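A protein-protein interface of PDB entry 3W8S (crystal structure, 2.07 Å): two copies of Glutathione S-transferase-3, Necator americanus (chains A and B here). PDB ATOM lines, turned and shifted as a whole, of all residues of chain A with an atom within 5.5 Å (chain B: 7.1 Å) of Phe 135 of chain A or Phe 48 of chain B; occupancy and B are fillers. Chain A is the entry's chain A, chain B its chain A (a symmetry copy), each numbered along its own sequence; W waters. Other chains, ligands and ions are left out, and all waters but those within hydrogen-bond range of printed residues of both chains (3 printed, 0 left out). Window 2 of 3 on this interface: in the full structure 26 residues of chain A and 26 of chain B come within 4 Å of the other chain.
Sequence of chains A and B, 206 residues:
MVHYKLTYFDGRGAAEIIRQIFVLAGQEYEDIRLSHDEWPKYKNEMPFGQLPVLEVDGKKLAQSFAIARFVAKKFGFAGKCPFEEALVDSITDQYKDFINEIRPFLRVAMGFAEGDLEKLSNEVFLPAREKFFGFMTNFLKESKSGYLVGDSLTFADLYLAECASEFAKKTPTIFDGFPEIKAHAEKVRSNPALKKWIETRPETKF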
ATOM      1  N   SER A  90      16.270 -19.088  19.041  1.00  0.00           N
ATOM      2  CA  SER A  90      16.675 -20.493  19.384  1.00  0.00           C
ATOM      3  C   SER A  90      18.146 -20.451  19.858  1.00  0.00           C
ATOM      4  O   SER A  90      18.551 -21.134  20.794  1.00  0.00           O
ATOM      5  CB  SER A  90      16.515 -21.454  18.152  1.00  0.00           C
ATOM      6  OG  SER A  90      17.556 -21.282  17.151  1.00  0.00           O
ATOM      7  N   ILE A  91      18.960 -19.603  19.203  1.00  0.00           N
ATOM      8  CA  ILE A  91      20.362 -19.525  19.571  1.00  0.00           C
ATOM      9  C   ILE A  91      20.542 -18.913  20.968  1.00  0.00           C
ATOM     10  O   ILE A  91      21.384 -19.434  21.789  1.00  0.00           O
ATOM     11  CB  ILE A  91      21.234 -18.698  18.526  1.00  0.00           C
ATOM     12  CG1 ILE A  91      21.466 -19.515  17.224  1.00  0.00           C
ATOM     13  CG2 ILE A  91      22.554 -18.306  19.194  1.00  0.00           C
ATOM     14  CD1 ILE A  91      21.983 -18.649  16.062  1.00  0.00           C
ATOM     15  N   GLN A  94      19.573 -21.532  23.463  1.00  0.00           N
ATOM     16  CA  GLN A  94      20.672 -22.504  23.671  1.00  0.00           C
ATOM     17  C   GLN A  94      21.814 -21.949  24.571  1.00  0.00           C
ATOM     18  O   GLN A  94      22.482 -22.681  25.329  1.00  0.00           O
ATOM     19  CB  GLN A  94      21.251 -22.968  22.297  1.00  0.00           C
ATOM     20  CG  GLN A  94      22.287 -24.144  22.378  1.00  0.00           C
ATOM     21  CD  GLN A  94      21.675 -25.434  22.959  1.00  0.00           C
ATOM     22  OE1 GLN A  94      20.430 -25.654  22.928  1.00  0.00           O
ATOM     23  NE2 GLN A  94      22.547 -26.341  23.428  1.00  0.00           N
ATOM     24  N   GLU A 130      32.684 -26.644  24.521  1.00  0.00           N
ATOM     25  CA  GLU A 130      32.930 -27.465  23.309  1.00  0.00           C
ATOM     26  C   GLU A 130      31.600 -27.819  22.583  1.00  0.00           C
ATOM     27  O   GLU A 130      31.502 -27.758  21.348  1.00  0.00           O
ATOM     28  CB  GLU A 130      33.672 -28.769  23.647  1.00  0.00           C
ATOM     29  CG  GLU A 130      33.762 -29.743  22.497  1.00  0.00           C
ATOM     30  CD  GLU A 130      34.608 -31.008  22.806  1.00  0.00           C
ATOM     31  OE1 GLU A 130      35.781 -30.881  23.297  1.00  0.00           O
ATOM     32  OE2 GLU A 130      34.075 -32.121  22.578  1.00  0.00           O
ATOM     33  N   LYS A 131      30.607 -28.254  23.338  1.00  0.00           N
ATOM     34  CA  LYS A 131      29.365 -28.595  22.676  1.00  0.00           C
ATOM     35  C   LYS A 131      28.708 -27.311  22.111  1.00  0.00           C
ATOM     36  O   LYS A 131      28.188 -27.317  20.972  1.00  0.00           O
ATOM     37  CB  LYS A 131      28.366 -29.160  23.695  1.00  0.00           C
ATOM     38  CG  LYS A 131      28.915 -30.445  24.308  1.00  0.00           C
ATOM     39  CD  LYS A 131      27.912 -31.095  25.270  1.00  0.00           C
ATOM     40  CE  LYS A 131      27.947 -30.320  26.588  1.00  0.00           C
ATOM     41  NZ  LYS A 131      27.256 -31.077  27.657  1.00  0.00           N
ATOM     42  N   PHE A 132      28.680 -26.263  22.940  1.00  0.00           N
ATOM     43  CA  PHE A 132      27.976 -24.997  22.523  1.00  0.00           C
ATOM     44  C   PHE A 132      28.693 -24.352  21.279  1.00  0.00           C
ATOM     45  O   PHE A 132      28.057 -24.025  20.242  1.00  0.00           O
ATOM     46  CB  PHE A 132      27.855 -24.034  23.710  1.00  0.00           C
ATOM     47  CG  PHE A 132      27.285 -22.695  23.335  1.00  0.00           C
ATOM     48  CD1 PHE A 132      25.938 -22.594  22.885  1.00  0.00           C
ATOM     49  CD2 PHE A 132      28.058 -21.525  23.448  1.00  0.00           C
ATOM     50  CE1 PHE A 132      25.405 -21.368  22.508  1.00  0.00           C
ATOM     51  CE2 PHE A 132      27.511 -20.278  23.069  1.00  0.00           C
ATOM     52  CZ  PHE A 132      26.175 -20.204  22.627  1.00  0.00           C
ATOM     53  N   PHE A 133      30.016 -24.223  21.344  1.00  0.00           N
ATOM     54  CA  PHE A 133      30.787 -23.707  20.209  1.00  0.00           C
ATOM     55  C   PHE A 133      30.653 -24.603  18.969  1.00  0.00           C
ATOM     56  O   PHE A 133      30.701 -24.121  17.840  1.00  0.00           O
ATOM     57  CB  PHE A 133      32.292 -23.584  20.563  1.00  0.00           C
ATOM     58  CG  PHE A 133      32.655 -22.361  21.350  1.00  0.00           C
ATOM     59  CD1 PHE A 133      31.643 -21.584  21.985  1.00  0.00           C
ATOM     60  CD2 PHE A 133      34.019 -21.978  21.491  1.00  0.00           C
ATOM     61  CE1 PHE A 133      31.977 -20.463  22.726  1.00  0.00           C
ATOM     62  CE2 PHE A 133      34.354 -20.879  22.280  1.00  0.00           C
ATOM     63  CZ  PHE A 133      33.333 -20.099  22.862  1.00  0.00           C
ATOM     64  N   GLY A 134      30.496 -25.906  19.146  1.00  0.00           N
ATOM     65  CA  GLY A 134      30.295 -26.752  17.975  1.00  0.00           C
ATOM     66  C   GLY A 134      28.960 -26.437  17.332  1.00  0.00           C
ATOM     67  O   GLY A 134      28.885 -26.314  16.127  1.00  0.00           O
ATOM     68  N   PHE A 135      27.902 -26.280  18.107  1.00  0.00           N
ATOM     69  CA  PHE A 135      26.615 -25.887  17.447  1.00  0.00           C
ATOM     70  C   PHE A 135      26.708 -24.503  16.815  1.00  0.00           C
ATOM     71  O   PHE A 135      26.124 -24.297  15.760  1.00  0.00           O
ATOM     72  CB  PHE A 135      25.443 -25.905  18.453  1.00  0.00           C
ATOM     73  CG  PHE A 135      25.180 -27.295  19.018  1.00  0.00           C
ATOM     74  CD1 PHE A 135      25.141 -28.398  18.165  1.00  0.00           C
ATOM     75  CD2 PHE A 135      24.942 -27.483  20.388  1.00  0.00           C
ATOM     76  CE1 PHE A 135      24.906 -29.688  18.660  1.00  0.00           C
ATOM     77  CE2 PHE A 135      24.652 -28.774  20.904  1.00  0.00           C
ATOM     78  CZ  PHE A 135      24.660 -29.855  20.041  1.00  0.00           C
ATOM     79  N   MET A 136      27.330 -23.539  17.497  1.00  0.00           N
ATOM     80  CA  MET A 136      27.424 -22.173  16.932  1.00  0.00           C
ATOM     81  C   MET A 136      28.244 -22.194  15.647  1.00  0.00           C
ATOM     82  O   MET A 136      27.924 -21.475  14.669  1.00  0.00           O
ATOM     83  CB  MET A 136      28.089 -21.204  17.908  1.00  0.00           C
ATOM     84  CG  MET A 136      27.264 -20.956  19.200  1.00  0.00           C
ATOM     85  SD  MET A 136      25.572 -20.361  18.847  1.00  0.00           S
ATOM     86  CE  MET A 136      24.608 -21.924  18.798  1.00  0.00           C
ATOM     87  N   THR A 137      29.340 -22.964  15.658  1.00  0.00           N
ATOM     88  CA  THR A 137      30.125 -23.115  14.410  1.00  0.00           C
ATOM     89  C   THR A 137      29.339 -23.701  13.234  1.00  0.00           C
ATOM     90  O   THR A 137      29.541 -23.282  12.082  1.00  0.00           O
ATOM     91  CB  THR A 137      31.402 -23.983  14.646  1.00  0.00           C
ATOM     92  OG1 THR A 137      32.174 -23.414  15.725  1.00  0.00           O
ATOM     93  CG2 THR A 137      32.283 -24.036  13.324  1.00  0.00           C
ATOM     94  N   ASN A 138      28.423 -24.648  13.472  1.00  0.00           N
ATOM     95  CA  ASN A 138      27.571 -25.137  12.328  1.00  0.00           C
ATOM     96  C   ASN A 138      26.753 -23.967  11.765  1.00  0.00           C
ATOM     97  O   ASN A 138      26.530 -23.870  10.569  1.00  0.00           O
ATOM     98  CB  ASN A 138      26.572 -26.174  12.805  1.00  0.00           C
ATOM     99  CG  ASN A 138      27.222 -27.411  13.320  1.00  0.00           C
ATOM    100  OD1 ASN A 138      28.417 -27.674  13.052  1.00  0.00           O
ATOM    101  ND2 ASN A 138      26.446 -28.201  14.112  1.00  0.00           N
ATOM    102  N   PHE A 139      26.229 -23.096  12.648  1.00  0.00           N
ATOM    103  CA  PHE A 139      25.511 -21.899  12.102  1.00  0.00           C
ATOM    104  C   PHE A 139      26.456 -21.018  11.255  1.00  0.00           C
ATOM    105  O   PHE A 139      26.089 -20.582  10.195  1.00  0.00           O
ATOM    106  CB  PHE A 139      24.863 -21.036  13.179  1.00  0.00           C
ATOM    107  CG  PHE A 139      23.538 -21.525  13.621  1.00  0.00           C
ATOM    108  CD1 PHE A 139      22.398 -21.091  12.969  1.00  0.00           C
ATOM    109  CD2 PHE A 139      23.410 -22.388  14.717  1.00  0.00           C
ATOM    110  CE1 PHE A 139      21.149 -21.495  13.401  1.00  0.00           C
ATOM    111  CE2 PHE A 139      22.168 -22.811  15.173  1.00  0.00           C
ATOM    112  CZ  PHE A 139      21.013 -22.353  14.521  1.00  0.00           C
ATOM    113  N   TRP B  39      15.757 -42.819  18.986  1.00  0.00           N
ATOM    114  CA  TRP B  39      16.276 -41.445  19.204  1.00  0.00           C
ATOM    115  C   TRP B  39      17.719 -41.266  18.724  1.00  0.00           C
ATOM    116  O   TRP B  39      17.984 -40.345  17.981  1.00  0.00           O
ATOM    117  CB  TRP B  39      16.094 -41.038  20.686  1.00  0.00           C
ATOM    118  CG  TRP B  39      16.824 -39.768  21.068  1.00  0.00           C
ATOM    119  CD1 TRP B  39      17.703 -39.623  22.166  1.00  0.00           C
ATOM    120  CD2 TRP B  39      16.742 -38.483  20.438  1.00  0.00           C
ATOM    121  NE1 TRP B  39      18.179 -38.315  22.205  1.00  0.00           N
ATOM    122  CE2 TRP B  39      17.636 -37.611  21.146  1.00  0.00           C
ATOM    123  CE3 TRP B  39      16.076 -37.983  19.279  1.00  0.00           C
ATOM    124  CZ2 TRP B  39      17.786 -36.252  20.813  1.00  0.00           C
ATOM    125  CZ3 TRP B  39      16.258 -36.627  18.935  1.00  0.00           C
ATOM    126  CH2 TRP B  39      17.097 -35.780  19.691  1.00  0.00           C
ATOM    127  N   LYS B  43      18.928 -38.015  16.480  1.00  0.00           N
ATOM    128  CA  LYS B  43      19.474 -36.924  17.286  1.00  0.00           C
ATOM    129  C   LYS B  43      20.293 -35.982  16.439  1.00  0.00           C
ATOM    130  O   LYS B  43      20.163 -34.740  16.544  1.00  0.00           O
ATOM    131  CB  LYS B  43      20.305 -37.548  18.415  1.00  0.00           C
ATOM    132  CG  LYS B  43      21.055 -36.567  19.321  1.00  0.00           C
ATOM    133  CD  LYS B  43      21.465 -37.333  20.589  1.00  0.00           C
ATOM    134  CE  LYS B  43      22.434 -36.509  21.430  1.00  0.00           C
ATOM    135  NZ  LYS B  43      21.596 -35.557  22.223  1.00  0.00           N
ATOM    136  N   GLU B  45      19.965 -35.061  13.420  1.00  0.00           N
ATOM    137  CA  GLU B  45      19.238 -34.121  12.543  1.00  0.00           C
ATOM    138  C   GLU B  45      18.747 -32.885  13.282  1.00  0.00           C
ATOM    139  O   GLU B  45      18.298 -31.909  12.672  1.00  0.00           O
ATOM    140  CB  GLU B  45      18.009 -34.775  11.932  1.00  0.00           C
ATOM    141  CG  GLU B  45      18.321 -36.026  11.117  1.00  0.00           C
ATOM    142  CD  GLU B  45      17.017 -36.724  10.723  1.00  0.00           C
ATOM    143  OE1 GLU B  45      15.949 -36.113  10.897  1.00  0.00           O
ATOM    144  OE2 GLU B  45      17.035 -37.874  10.259  1.00  0.00           O
ATOM    145  N   MET B  46      18.879 -32.881  14.599  1.00  0.00           N
ATOM    146  CA  MET B  46      18.347 -31.736  15.344  1.00  0.00           C
ATOM    147  C   MET B  46      19.416 -30.655  15.548  1.00  0.00           C
ATOM    148  O   MET B  46      20.508 -30.957  15.956  1.00  0.00           O
ATOM    149  CB  MET B  46      17.779 -32.238  16.655  1.00  0.00           C
ATOM    150  CG  MET B  46      16.938 -33.517  16.476  1.00  0.00           C
ATOM    151  SD  MET B  46      15.528 -33.247  15.287  1.00  0.00           S
ATOM    152  CE  MET B  46      14.973 -34.968  15.076  1.00  0.00           C
ATOM    153  N   PRO B  47      19.065 -29.385  15.359  1.00  0.00           N
ATOM    154  CA  PRO B  47      20.068 -28.316  15.511  1.00  0.00           C
ATOM    155  C   PRO B  47      20.917 -28.358  16.782  1.00  0.00           C
ATOM    156  O   PRO B  47      22.114 -28.091  16.686  1.00  0.00           O
ATOM    157  CB  PRO B  47      19.232 -27.039  15.443  1.00  0.00           C
ATOM    158  CG  PRO B  47      18.043 -27.445  14.531  1.00  0.00           C
ATOM    159  CD  PRO B  47      17.712 -28.842  15.077  1.00  0.00           C
ATOM    160  N   PHE B  48      20.337 -28.645  17.948  1.00  0.00           N
ATOM    161  CA  PHE B  48      21.181 -28.766  19.159  1.00  0.00           C
ATOM    162  C   PHE B  48      21.151 -30.169  19.765  1.00  0.00           C
ATOM    163  O   PHE B  48      21.399 -30.309  20.957  1.00  0.00           O
ATOM    164  CB  PHE B  48      20.867 -27.694  20.200  1.00  0.00           C
ATOM    165  CG  PHE B  48      20.720 -26.283  19.605  1.00  0.00           C
ATOM    166  CD1 PHE B  48      21.813 -25.641  19.026  1.00  0.00           C
ATOM    167  CD2 PHE B  48      19.493 -25.597  19.659  1.00  0.00           C
ATOM    168  CE1 PHE B  48      21.710 -24.340  18.471  1.00  0.00           C
ATOM    169  CE2 PHE B  48      19.356 -24.294  19.144  1.00  0.00           C
ATOM    170  CZ  PHE B  48      20.461 -23.663  18.511  1.00  0.00           C
ATOM    171  N   GLY B  49      20.936 -31.191  18.925  1.00  0.00           N
ATOM    172  CA  GLY B  49      20.933 -32.615  19.371  1.00  0.00           C
ATOM    173  C   GLY B  49      19.784 -32.853  20.349  1.00  0.00           C
ATOM    174  O   GLY B  49      19.841 -33.831  21.117  1.00  0.00           O
ATOM    175  N   GLN B  50      18.719 -32.008  20.345  1.00  0.00           N
ATOM    176  CA  GLN B  50      17.635 -32.182  21.362  1.00  0.00           C
ATOM    177  C   GLN B  50      16.212 -31.934  20.782  1.00  0.00           C
ATOM    178  O   GLN B  50      16.103 -31.451  19.672  1.00  0.00           O
ATOM    179  CB  GLN B  50      17.871 -31.266  22.594  1.00  0.00           C
ATOM    180  CG  GLN B  50      19.140 -31.692  23.400  1.00  0.00           C
ATOM    181  CD  GLN B  50      19.121 -31.099  24.752  1.00  0.00           C
ATOM    182  OE1 GLN B  50      19.128 -29.851  24.897  1.00  0.00           O
ATOM    183  NE2 GLN B  50      19.049 -31.960  25.783  1.00  0.00           N
ATOM    184  N   LEU B  51      15.151 -32.213  21.570  1.00  0.00           N
ATOM    185  CA  LEU B  51      13.772 -32.020  21.108  1.00  0.00           C
ATOM    186  C   LEU B  51      13.130 -31.116  22.108  1.00  0.00           C
ATOM    187  O   LEU B  51      13.538 -31.127  23.269  1.00  0.00           O
ATOM    188  CB  LEU B  51      13.088 -33.401  20.999  1.00  0.00           C
ATOM    189  CG  LEU B  51      13.688 -34.351  19.945  1.00  0.00           C
ATOM    190  CD1 LEU B  51      12.939 -35.692  20.052  1.00  0.00           C
ATOM    191  CD2 LEU B  51      13.624 -33.788  18.519  1.00  0.00           C
ATOM    192  N   VAL B  53      11.778 -30.095  18.028  1.00  0.00           N
ATOM    193  CA  VAL B  53      12.211 -29.373  16.833  1.00  0.00           C
ATOM    194  C   VAL B  53      10.982 -29.182  15.924  1.00  0.00           C
ATOM    195  O   VAL B  53      10.225 -30.114  15.667  1.00  0.00           O
ATOM    196  CB  VAL B  53      13.310 -30.126  16.060  1.00  0.00           C
ATOM    197  CG1 VAL B  53      13.598 -29.456  14.675  1.00  0.00           C
ATOM    198  CG2 VAL B  53      14.606 -30.158  16.885  1.00  0.00           C
ATOM    199  N   LEU B  61      13.852 -25.616  13.199  1.00  0.00           N
ATOM    200  CA  LEU B  61      13.913 -24.651  14.305  1.00  0.00           C
ATOM    201  C   LEU B  61      13.824 -25.470  15.601  1.00  0.00           C
ATOM    202  O   LEU B  61      12.858 -26.236  15.831  1.00  0.00           O
ATOM    203  CB  LEU B  61      12.777 -23.647  14.201  1.00  0.00           C
ATOM    204  CG  LEU B  61      12.524 -22.658  15.386  1.00  0.00           C
ATOM    205  CD1 LEU B  61      13.684 -21.665  15.494  1.00  0.00           C
ATOM    206  CD2 LEU B  61      11.148 -21.974  15.213  1.00  0.00           C
ATOM    207  N   ALA B  62      14.835 -25.268  16.465  1.00  0.00           N
ATOM    208  CA  ALA B  62      14.895 -25.880  17.795  1.00  0.00           C
ATOM    209  C   ALA B  62      14.472 -24.893  18.872  1.00  0.00           C
ATOM    210  O   ALA B  62      14.243 -23.684  18.590  1.00  0.00           O
ATOM    211  CB  ALA B  62      16.341 -26.344  18.070  1.00  0.00           C
ATOM    212  N   GLN B  63      14.379 -25.410  20.105  1.00  0.00           N
ATOM    213  CA  GLN B  63      14.217 -24.646  21.337  1.00  0.00           C
ATOM    214  C   GLN B  63      12.759 -24.376  21.569  1.00  0.00           C
ATOM    215  O   GLN B  63      12.210 -23.508  20.910  1.00  0.00           O
ATOM    216  CB  GLN B  63      15.122 -23.395  21.402  1.00  0.00           C
ATOM    217  CG  GLN B  63      16.602 -23.735  21.798  1.00  0.00           C
ATOM    218  CD  GLN B  63      16.753 -24.104  23.262  1.00  0.00           C
ATOM    219  OE1 GLN B  63      15.840 -23.937  24.104  1.00  0.00           O
ATOM    220  NE2 GLN B  63      17.904 -24.596  23.587  1.00  0.00           N
HETATM  221  O   HOH W   1      18.715 -27.737  23.488  1.00  0.00           O
HETATM  222  O   HOH W   2      17.347 -23.745  15.651  1.00  0.00           O
HETATM  223  O   HOH W   3      21.838 -29.218  23.357  1.00  0.00           O
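Phe 135 of chain A touches just these residues of chain B: Pro 47 and Phe 48.
Phe 48 of chain B touches just these residues of chain A: Ser 90, Gln 94, Phe 135, Met 136 and Phe 139.
No residue of chain B comes within 4 Å of Gly 134 of chain A.
Printed residues of chain B within 4 Å of Ser 90 of chain A: Phe 48, Leu 61, Ala 62 and Gln 63.
Of the printed residues of chain A, Ala 62 of chain B touches Ser 90.
The nearest residue of chain B that does not touch Phe 135 of chain A is Gly 49 of chain B (4.1 Å).
No position is printed for both chains.
Of the 10 pairs that touch across the chains among the printed residues, none has its exchanged pair printed and touching as well.
OE1 of Gln 94 of chain A is in hydrogen-bond range of NE2 of Gln 63 of chain B.
Phe 48 of chain B touches Ser 90 of chain A.
Leu 61 of chain B touches Ser 90 of chain A (CD1 to CB, 3.9 Å).
CB of Ser 90 of chain A touches O of Ala 62 of chain B, 3.2 Å away.
Gln 63 of chain B touches Ser 90 of chain A.
CG of Phe 48 of chain B touches OE1 of Gln 94 of chain A, at 3.4 Å.
Pro 47 of chain B touches Phe 135 of chain A.
Phe 48 of chain B touches Phe 135 of chain A.
CE of Met 136 of chain A touches CE1 of Phe 48 of chain B, at 3.8 Å.
Phe 139 of chain A touches Phe 48 of chain B (CE2 to CE1, 3.7 Å).
Of the 13 printed residues of chain A, 5 touch a printed residue of chain B.
Hydrophobic or aromatic side chains of chain A that line the printed part of chain B: Phe 135, Met 136 and Phe 139.
Along chain A the printed residues that touch a printed residue of chain B span positions 90 to 139.
Along chain B the printed residues that touch a printed residue of chain A span positions 47 to 63.
Water W1 lies within hydrogen-bond range of OE1 of Gln 50 of chain B (2.6 Å), OE1 of Gln 94 of chain A (2.8 Å) and NE2 of Gln 63 of chain B (3.2 Å).
Water W3 lies within hydrogen-bond range of O of Phe 48 of chain B, NE2 of Gln 94 of chain A and OE1 of Gln 50 of chain B.
Water W2 bridges the side-chain hydroxyl (OG) of Ser 90 of chain A (2.9 Å) and the backbone NH (N) of Ala 62 of chain B (3.0 Å).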
